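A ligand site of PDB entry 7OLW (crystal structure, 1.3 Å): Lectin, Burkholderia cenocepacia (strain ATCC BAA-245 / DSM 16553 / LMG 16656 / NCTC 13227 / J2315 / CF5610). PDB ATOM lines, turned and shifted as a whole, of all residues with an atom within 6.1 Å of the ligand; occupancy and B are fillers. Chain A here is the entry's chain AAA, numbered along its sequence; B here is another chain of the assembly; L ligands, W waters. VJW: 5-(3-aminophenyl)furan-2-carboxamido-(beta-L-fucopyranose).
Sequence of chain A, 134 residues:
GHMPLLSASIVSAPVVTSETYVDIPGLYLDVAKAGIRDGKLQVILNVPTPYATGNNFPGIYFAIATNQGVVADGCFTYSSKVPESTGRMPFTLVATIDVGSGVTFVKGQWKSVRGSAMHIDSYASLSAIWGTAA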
ATOM      1  N   TYR A  21       7.985 -28.071  30.073  1.00  0.00           N
ATOM      2  CA  TYR A  21       8.193 -29.489  29.746  1.00  0.00           C
ATOM      3  C   TYR A  21       7.367 -30.356  30.673  1.00  0.00           C
ATOM      4  O   TYR A  21       7.446 -30.206  31.893  1.00  0.00           O
ATOM      5  CB  TYR A  21       9.680 -29.856  29.776  1.00  0.00           C
ATOM      6  CG  TYR A  21      10.386 -29.401  28.529  1.00  0.00           C
ATOM      7  CD1 TYR A  21      10.026 -29.899  27.284  1.00  0.00           C
ATOM      8  CD2 TYR A  21      11.371 -28.443  28.608  1.00  0.00           C
ATOM      9  CE1 TYR A  21      10.634 -29.422  26.141  1.00  0.00           C
ATOM     10  CE2 TYR A  21      11.991 -27.985  27.466  1.00  0.00           C
ATOM     11  CZ  TYR A  21      11.638 -28.489  26.226  1.00  0.00           C
ATOM     12  OH  TYR A  21      12.218 -28.010  25.077  1.00  0.00           O
ATOM     13  N   PHE A  57       1.936 -20.315  13.873  1.00  0.00           N
ATOM     14  CA  PHE A  57       3.158 -21.063  13.486  1.00  0.00           C
ATOM     15  C   PHE A  57       3.401 -22.208  14.473  1.00  0.00           C
ATOM     16  O   PHE A  57       4.316 -22.193  15.277  1.00  0.00           O
ATOM     17  CB  PHE A  57       4.373 -20.122  13.418  1.00  0.00           C
ATOM     18  CG  PHE A  57       4.221 -19.071  12.360  1.00  0.00           C
ATOM     19  CD1 PHE A  57       4.669 -19.302  11.074  1.00  0.00           C
ATOM     20  CD2 PHE A  57       3.697 -17.830  12.670  1.00  0.00           C
ATOM     21  CE1 PHE A  57       4.546 -18.318  10.096  1.00  0.00           C
ATOM     22  CE2 PHE A  57       3.559 -16.862  11.688  1.00  0.00           C
ATOM     23  CZ  PHE A  57       4.003 -17.100  10.418  1.00  0.00           C
ATOM     24  N   PRO A  58       2.540 -23.248  14.427  1.00  0.00           N
ATOM     25  CA  PRO A  58       2.558 -24.270  15.473  1.00  0.00           C
ATOM     26  C   PRO A  58       3.831 -25.123  15.477  1.00  0.00           C
ATOM     27  O   PRO A  58       4.570 -25.197  14.478  1.00  0.00           O
ATOM     28  CB  PRO A  58       1.336 -25.145  15.168  1.00  0.00           C
ATOM     29  CG  PRO A  58       0.436 -24.237  14.354  1.00  0.00           C
ATOM     30  CD  PRO A  58       1.410 -23.419  13.536  1.00  0.00           C
ATOM     31  N   TYR A  61       8.093 -28.542  21.249  1.00  0.00           N
ATOM     32  CA  TYR A  61       9.419 -28.779  21.827  1.00  0.00           C
ATOM     33  C   TYR A  61       9.428 -30.161  22.455  1.00  0.00           C
ATOM     34  O   TYR A  61       8.448 -30.529  23.113  1.00  0.00           O
ATOM     35  CB  TYR A  61       9.737 -27.797  22.958  1.00  0.00           C
ATOM     36  CG  TYR A  61       9.893 -26.353  22.551  1.00  0.00           C
ATOM     37  CD1 TYR A  61      11.120 -25.872  22.129  1.00  0.00           C
ATOM     38  CD2 TYR A  61       8.867 -25.453  22.671  1.00  0.00           C
ATOM     39  CE1 TYR A  61      11.302 -24.556  21.782  1.00  0.00           C
ATOM     40  CE2 TYR A  61       9.036 -24.117  22.368  1.00  0.00           C
ATOM     41  CZ  TYR A  61      10.257 -23.671  21.884  1.00  0.00           C
ATOM     42  OH  TYR A  61      10.501 -22.387  21.505  1.00  0.00           O
ATOM     43  N   ASP A  73      17.233 -30.644  24.379  1.00  0.00           N
ATOM     44  CA  ASP A  73      15.879 -30.386  23.843  1.00  0.00           C
ATOM     45  C   ASP A  73      15.982 -29.870  22.416  1.00  0.00           C
ATOM     46  O   ASP A  73      17.074 -29.633  21.901  1.00  0.00           O
ATOM     47  CB  ASP A  73      15.048 -29.481  24.708  1.00  0.00           C
ATOM     48  CG  ASP A  73      15.463 -28.035  24.679  1.00  0.00           C
ATOM     49  OD1 ASP A  73      16.526 -27.711  24.130  1.00  0.00           O
ATOM     50  OD2 ASP A  73      14.673 -27.256  25.201  1.00  0.00           O
ATOM     51  N   GLY A  74      14.837 -29.793  21.760  1.00  0.00           N
ATOM     52  CA  GLY A  74      14.746 -29.251  20.409  1.00  0.00           C
ATOM     53  C   GLY A  74      13.300 -29.037  20.064  1.00  0.00           C
ATOM     54  O   GLY A  74      12.427 -29.248  20.913  1.00  0.00           O
ATOM     55  N   CYS A  75      13.033 -28.638  18.847  1.00  0.00           N
ATOM     56  CA  CYS A  75      11.626 -28.528  18.395  1.00  0.00           C
ATOM     57  C   CYS A  75      11.538 -28.688  16.885  1.00  0.00           C
ATOM     58  O   CYS A  75      12.537 -28.533  16.183  1.00  0.00           O
ATOM     59  CB  CYS A  75      10.978 -27.225  18.851  1.00  0.00           C
ATOM     60  SG  CYS A  75      11.459 -25.730  17.950  1.00  0.00           S
ATOM     61  N   THR A  77       8.901 -26.699  14.005  1.00  0.00           N
ATOM     62  CA  THR A  77       7.834 -25.705  13.789  1.00  0.00           C
ATOM     63  C   THR A  77       7.458 -25.689  12.320  1.00  0.00           C
ATOM     64  O   THR A  77       8.296 -25.973  11.452  1.00  0.00           O
ATOM     65  CB  THR A  77       8.197 -24.313  14.259  1.00  0.00           C
ATOM     66  OG1 THR A  77       9.363 -23.887  13.567  1.00  0.00           O
ATOM     67  CG2 THR A  77       8.432 -24.232  15.756  1.00  0.00           C
ATOM     68  N   TYR A  78       6.194 -25.390  12.043  1.00  0.00           N
ATOM     69  CA  TYR A  78       5.725 -25.182  10.655  1.00  0.00           C
ATOM     70  C   TYR A  78       6.240 -23.843  10.139  1.00  0.00           C
ATOM     71  O   TYR A  78       6.606 -22.952  10.906  1.00  0.00           O
ATOM     72  CB  TYR A  78       4.205 -25.294  10.608  1.00  0.00           C
ATOM     73  CG  TYR A  78       3.682 -26.643  10.976  1.00  0.00           C
ATOM     74  CD1 TYR A  78       3.935 -27.755  10.194  1.00  0.00           C
ATOM     75  CD2 TYR A  78       2.963 -26.847  12.149  1.00  0.00           C
ATOM     76  CE1 TYR A  78       3.467 -29.009  10.547  1.00  0.00           C
ATOM     77  CE2 TYR A  78       2.507 -28.092  12.521  1.00  0.00           C
ATOM     78  CZ  TYR A  78       2.738 -29.182  11.711  1.00  0.00           C
ATOM     79  OH  TYR A  78       2.307 -30.413  12.114  1.00  0.00           O
ATOM     80  N   LYS A 111       6.581 -29.798  25.230  1.00  0.00           N
ATOM     81  CA  LYS A 111       6.070 -28.464  25.591  1.00  0.00           C
ATOM     82  C   LYS A 111       5.579 -27.804  24.313  1.00  0.00           C
ATOM     83  O   LYS A 111       6.154 -28.016  23.234  1.00  0.00           O
ATOM     84  CB  LYS A 111       7.199 -27.670  26.264  1.00  0.00           C
ATOM     85  CG  LYS A 111       6.977 -26.214  26.495  1.00  0.00           C
ATOM     86  CD  LYS A 111       8.158 -25.580  27.156  1.00  0.00           C
ATOM     87  CE  LYS A 111       9.474 -25.639  26.429  1.00  0.00           C
ATOM     88  NZ  LYS A 111      10.456 -24.709  27.068  1.00  0.00           N
ATOM     89  N   VAL A 113       4.865 -25.092  21.373  1.00  0.00           N
ATOM     90  CA  VAL A 113       5.336 -23.845  20.741  1.00  0.00           C
ATOM     91  C   VAL A 113       4.099 -22.969  20.562  1.00  0.00           C
ATOM     92  O   VAL A 113       3.117 -23.406  19.938  1.00  0.00           O
ATOM     93  CB  VAL A 113       6.019 -24.089  19.389  1.00  0.00           C
ATOM     94  CG1 VAL A 113       6.403 -22.765  18.757  1.00  0.00           C
ATOM     95  CG2 VAL A 113       7.217 -25.044  19.505  1.00  0.00           C
ATOM     96  N   ARG A 114       4.103 -21.768  21.147  1.00  0.00           N
ATOM     97  CA  ARG A 114       3.023 -20.800  20.910  1.00  0.00           C
ATOM     98  C   ARG A 114       1.638 -21.433  21.143  1.00  0.00           C
ATOM     99  O   ARG A 114       0.747 -21.259  20.344  1.00  0.00           O
ATOM    100  CB  ARG A 114       3.188 -20.131  19.539  1.00  0.00           C
ATOM    101  CG  ARG A 114       4.395 -19.223  19.455  1.00  0.00           C
ATOM    102  CD  ARG A 114       4.631 -18.624  18.090  1.00  0.00           C
ATOM    103  NE  ARG A 114       5.084 -19.614  17.118  1.00  0.00           N
ATOM    104  CZ  ARG A 114       6.360 -19.914  16.889  1.00  0.00           C
ATOM    105  NH1 ARG A 114       7.332 -19.303  17.534  1.00  0.00           N
ATOM    106  NH2 ARG A 114       6.655 -20.821  15.987  1.00  0.00           N
ATOM    107  N   THR B  49      17.079 -28.915  15.677  1.00  0.00           N
ATOM    108  CA  THR B  49      16.337 -27.646  15.561  1.00  0.00           C
ATOM    109  C   THR B  49      17.035 -26.654  14.645  1.00  0.00           C
ATOM    110  O   THR B  49      17.097 -25.465  14.962  1.00  0.00           O
ATOM    111  CB  THR B  49      16.074 -27.024  16.939  1.00  0.00           C
ATOM    112  OG1 THR B  49      15.796 -28.035  17.914  1.00  0.00           O
ATOM    113  CG2 THR B  49      14.901 -26.072  16.911  1.00  0.00           C
ATOM    114  N   TYR B  51      17.552 -24.169  11.258  1.00  0.00           N
ATOM    115  CA  TYR B  51      16.789 -23.494  10.193  1.00  0.00           C
ATOM    116  C   TYR B  51      17.748 -22.872   9.209  1.00  0.00           C
ATOM    117  O   TYR B  51      18.929 -22.679   9.515  1.00  0.00           O
ATOM    118  CB  TYR B  51      15.762 -22.496  10.736  1.00  0.00           C
ATOM    119  CG  TYR B  51      16.310 -21.242  11.377  1.00  0.00           C
ATOM    120  CD1 TYR B  51      16.771 -21.250  12.676  1.00  0.00           C
ATOM    121  CD2 TYR B  51      16.296 -20.046  10.685  1.00  0.00           C
ATOM    122  CE1 TYR B  51      17.185 -20.083  13.292  1.00  0.00           C
ATOM    123  CE2 TYR B  51      16.686 -18.870  11.280  1.00  0.00           C
ATOM    124  CZ  TYR B  51      17.146 -18.895  12.578  1.00  0.00           C
ATOM    125  OH  TYR B  51      17.538 -17.724  13.165  1.00  0.00           O
ATOM    126  N   TYR B  78      13.085 -26.504   2.521  1.00  0.00           N
ATOM    127  CA  TYR B  78      11.691 -26.014   2.594  1.00  0.00           C
ATOM    128  C   TYR B  78      10.981 -26.305   1.279  1.00  0.00           C
ATOM    129  O   TYR B  78      11.606 -26.523   0.235  1.00  0.00           O
ATOM    130  CB  TYR B  78      11.686 -24.538   2.949  1.00  0.00           C
ATOM    131  CG  TYR B  78      12.259 -24.228   4.305  1.00  0.00           C
ATOM    132  CD1 TYR B  78      11.639 -24.664   5.457  1.00  0.00           C
ATOM    133  CD2 TYR B  78      13.458 -23.548   4.454  1.00  0.00           C
ATOM    134  CE1 TYR B  78      12.170 -24.406   6.708  1.00  0.00           C
ATOM    135  CE2 TYR B  78      14.014 -23.296   5.689  1.00  0.00           C
ATOM    136  CZ  TYR B  78      13.354 -23.717   6.826  1.00  0.00           C
ATOM    137  OH  TYR B  78      13.941 -23.483   8.041  1.00  0.00           O
ATOM    138  N   SER B  85       7.752 -18.140   7.333  1.00  0.00           N
ATOM    139  CA  SER B  85       8.693 -18.236   8.468  1.00  0.00           C
ATOM    140  C   SER B  85       9.537 -19.466   8.232  1.00  0.00           C
ATOM    141  O   SER B  85       9.010 -20.459   7.717  1.00  0.00           O
ATOM    142  CB  SER B  85       7.940 -18.341   9.753  1.00  0.00           C
ATOM    143  OG  SER B  85       8.787 -18.709  10.831  1.00  0.00           O
ATOM    144  N   THR B  86      10.838 -19.376   8.463  1.00  0.00           N
ATOM    145  CA  THR B  86      11.716 -20.548   8.266  1.00  0.00           C
ATOM    146  C   THR B  86      11.582 -21.457   9.481  1.00  0.00           C
ATOM    147  O   THR B  86      12.264 -21.243  10.497  1.00  0.00           O
ATOM    148  CB  THR B  86      13.147 -20.085   8.014  1.00  0.00           C
ATOM    149  OG1 THR B  86      13.573 -19.266   9.106  1.00  0.00           O
ATOM    150  CG2 THR B  86      13.272 -19.336   6.695  1.00  0.00           C
ATOM    151  N   GLY B  87      10.716 -22.439   9.375  1.00  0.00           N
ATOM    152  CA  GLY B  87      10.460 -23.343  10.511  1.00  0.00           C
ATOM    153  C   GLY B  87      11.668 -24.187  10.891  1.00  0.00           C
ATOM    154  O   GLY B  87      12.571 -24.434  10.080  1.00  0.00           O
ATOM    155  N   ARG B  88      11.596 -24.759  12.061  1.00  0.00           N
ATOM    156  CA  ARG B  88      12.653 -25.665  12.553  1.00  0.00           C
ATOM    157  C   ARG B  88      12.406 -27.057  11.968  1.00  0.00           C
ATOM    158  O   ARG B  88      11.326 -27.600  12.094  1.00  0.00           O
ATOM    159  CB  ARG B  88      12.661 -25.662  14.065  1.00  0.00           C
ATOM    160  CG  ARG B  88      12.860 -24.293  14.693  1.00  0.00           C
ATOM    161  CD  ARG B  88      14.010 -23.503  14.106  1.00  0.00           C
ATOM    162  NE  ARG B  88      14.261 -22.247  14.786  1.00  0.00           N
ATOM    163  CZ  ARG B  88      15.269 -21.948  15.581  1.00  0.00           C
ATOM    164  NH1 ARG B  88      16.207 -22.823  15.884  1.00  0.00           N
ATOM    165  NH2 ARG B  88      15.348 -20.746  16.082  1.00  0.00           N
ATOM    166  N   ASP B 121      21.050 -22.606  16.931  1.00  0.00           N
ATOM    167  CA  ASP B 121      20.927 -21.704  18.097  1.00  0.00           C
ATOM    168  C   ASP B 121      20.358 -22.471  19.271  1.00  0.00           C
ATOM    169  O   ASP B 121      19.877 -21.866  20.203  1.00  0.00           O
ATOM    170  CB  ASP B 121      20.079 -20.474  17.765  1.00  0.00           C
ATOM    171  CG  ASP B 121      18.645 -20.795  17.433  1.00  0.00           C
ATOM    172  OD1 ASP B 121      18.281 -21.993  17.435  1.00  0.00           O
ATOM    173  OD2 ASP B 121      17.884 -19.843  17.155  1.00  0.00           O
ATOM    174  N   SER B 122      20.485 -23.787  19.259  1.00  0.00           N
ATOM    175  CA  SER B 122      20.051 -24.613  20.382  1.00  0.00           C
ATOM    176  C   SER B 122      20.822 -25.937  20.287  1.00  0.00           C
ATOM    177  O   SER B 122      21.633 -26.117  19.387  1.00  0.00           O
ATOM    178  CB  SER B 122      18.553 -24.799  20.371  1.00  0.00           C
ATOM    179  OG  SER B 122      18.114 -25.496  19.214  1.00  0.00           O
ATOM    180  N   TYR B 123      20.552 -26.856  21.194  1.00  0.00           N
ATOM    181  CA  TYR B 123      21.271 -28.124  21.318  1.00  0.00           C
ATOM    182  C   TYR B 123      21.419 -28.838  19.969  1.00  0.00           C
ATOM    183  O   TYR B 123      20.443 -29.021  19.213  1.00  0.00           O
ATOM    184  CB  TYR B 123      20.519 -29.029  22.291  1.00  0.00           C
ATOM    185  CG  TYR B 123      21.146 -30.373  22.520  1.00  0.00           C
ATOM    186  CD1 TYR B 123      20.798 -31.429  21.691  1.00  0.00           C
ATOM    187  CD2 TYR B 123      22.078 -30.572  23.505  1.00  0.00           C
ATOM    188  CE1 TYR B 123      21.377 -32.685  21.871  1.00  0.00           C
ATOM    189  CE2 TYR B 123      22.646 -31.823  23.704  1.00  0.00           C
ATOM    190  CZ  TYR B 123      22.280 -32.879  22.896  1.00  0.00           C
ATOM    191  OH  TYR B 123      22.825 -34.129  23.103  1.00  0.00           O
HETATM  192  N1  VJW L   1      12.554 -20.135  17.411  1.00  0.00           N
HETATM  193  C4  VJW L   1      11.141 -20.095  13.489  1.00  0.00           C
HETATM  194  C5  VJW L   1      12.213 -19.116  13.946  1.00  0.00           C
HETATM  195  C6  VJW L   1      13.327 -18.958  12.950  1.00  0.00           C
HETATM  196  C7  VJW L   1      13.374 -19.323  18.077  1.00  0.00           C
HETATM  197  C8  VJW L   1      14.186 -19.934  19.111  1.00  0.00           C
HETATM  198  C10 VJW L   1      15.524 -20.501  20.804  1.00  0.00           C
HETATM  199  C13 VJW L   1      15.024 -23.238  22.208  1.00  0.00           C
HETATM  200  C15 VJW L   1      14.851 -25.562  21.806  1.00  0.00           C
HETATM  201  C17 VJW L   1      14.653 -24.039  19.989  1.00  0.00           C
HETATM  202  C1  VJW L   1      11.851 -19.702  16.255  1.00  0.00           C
HETATM  203  O5  VJW L   1      12.780 -19.615  15.171  1.00  0.00           O
HETATM  204  C3  VJW L   1      10.099 -20.267  14.586  1.00  0.00           C
HETATM  205  O3  VJW L   1       9.127 -21.257  14.245  1.00  0.00           O
HETATM  206  C2  VJW L   1      10.759 -20.687  15.894  1.00  0.00           C
HETATM  207  O2  VJW L   1       9.758 -20.715  16.896  1.00  0.00           O
HETATM  208  O4  VJW L   1      11.741 -21.354  13.189  1.00  0.00           O
HETATM  209  O7  VJW L   1      13.497 -18.135  17.789  1.00  0.00           O
HETATM  210  O8  VJW L   1      14.020 -21.278  19.359  1.00  0.00           O
HETATM  211  C11 VJW L   1      14.843 -21.584  20.407  1.00  0.00           C
HETATM  212  C9  VJW L   1      15.090 -19.430  19.978  1.00  0.00           C
HETATM  213  C12 VJW L   1      14.849 -22.975  20.863  1.00  0.00           C
HETATM  214  C16 VJW L   1      14.664 -25.334  20.468  1.00  0.00           C
HETATM  215  C14 VJW L   1      15.025 -24.533  22.698  1.00  0.00           C
HETATM  216  N2  VJW L   1      15.132 -24.775  24.068  1.00  0.00           N
HETATM  217  O   HOH W   1       7.755 -20.801  12.153  1.00  0.00           O
HETATM  218  O   HOH W   2      10.996 -22.514  18.625  1.00  0.00           O
HETATM  219  O   HOH W   3      17.833 -24.166  24.529  1.00  0.00           O
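CE1 of Tyr 61 touches C15 of the ligand, 3.7 Å away. CA of Gly 74 touches C16 of the ligand (3.9 Å). CG2 of Thr 49 of chain B touches C16 of the ligand, 3.6 Å away. Tyr 51 of chain B touches the ligand. Ser 85 of chain B touches the ligand (OG to C4, 3.8 Å). Gly 87 of chain B touches the ligand. Asp 121 of chain B touches the ligand (OD2 to C9, 3.99 Å). Ser 122 of chain B touches the ligand (OG to C16, 3.7 Å). Within 4 Å of the ligand: Tyr 61, Asp 73, Gly 74, Thr 77, Arg 114, Thr 49 of chain B, Tyr 51 of chain B, Ser 85 of chain B, Thr 86 of chain B, Gly 87 of chain B, Arg 88 of chain B, Asp 121 of chain B and Ser 122 of chain B.
The side-chain hydroxyl of Thr 77 is in hydrogen-bond range of the backbone NH of Arg 88 of chain B (2.8 Å). The side-chain hydroxyl of Tyr 21 sits at hydrogen-bond distance from the side-chain carboxylate of Asp 73 (2.6 Å). NH2 of Arg 114 lies within hydrogen-bond range of O of Phe 57 (2.8 Å). The guanidinium group (NH1) of Arg 88 of chain B sits at hydrogen-bond distance from the backbone carbonyl oxygen (O) of Thr 49 of chain B. The side-chain carboxylate of Asp 121 of chain B lies within salt-bridge range of the guanidinium group of Arg 88 of chain B (2.7 Å). The backbone carbonyl oxygen (O) of Gly 87 of chain B is in hydrogen-bond range of the side-chain hydroxyl (OH) of Tyr 78 of chain B (2.6 Å). The side-chain hydroxyl (OG1) of Thr 49 of chain B lies within hydrogen-bond range of the backbone NH (N) of Cys 75, 3.0 Å away. N of Tyr 61 lies within hydrogen-bond range of O of Lys 111.
An oxygen (O3) of the ligand is in hydrogen-bond range of the side-chain hydroxyl (OG1) of Thr 77. An oxygen (O4) of the ligand is in hydrogen-bond range of the backbone carbonyl oxygen (O) of Thr 86 of chain B (2.7 Å). OD2 of Asp 73 lies within hydrogen-bond range of N2 of the ligand, 2.8 Å away. The guanidinium group of Arg 114 lies within hydrogen-bond range of an oxygen (O2) of the ligand (2.9 Å). The guanidinium group of Arg 88 of chain B sits at hydrogen-bond distance from an oxygen (O5) of the ligand (3.0 Å).
Water W1 lies within hydrogen-bond range of an oxygen (O3) of the ligand (2.5 Å), the side-chain hydroxyl of Ser 85 of chain B (2.7 Å) and the backbone carbonyl oxygen of Tyr 78 of chain A (2.7 Å). Water W2 lies within hydrogen-bond range of O2 of the ligand, OH of Tyr 61 and SG of Cys 75.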
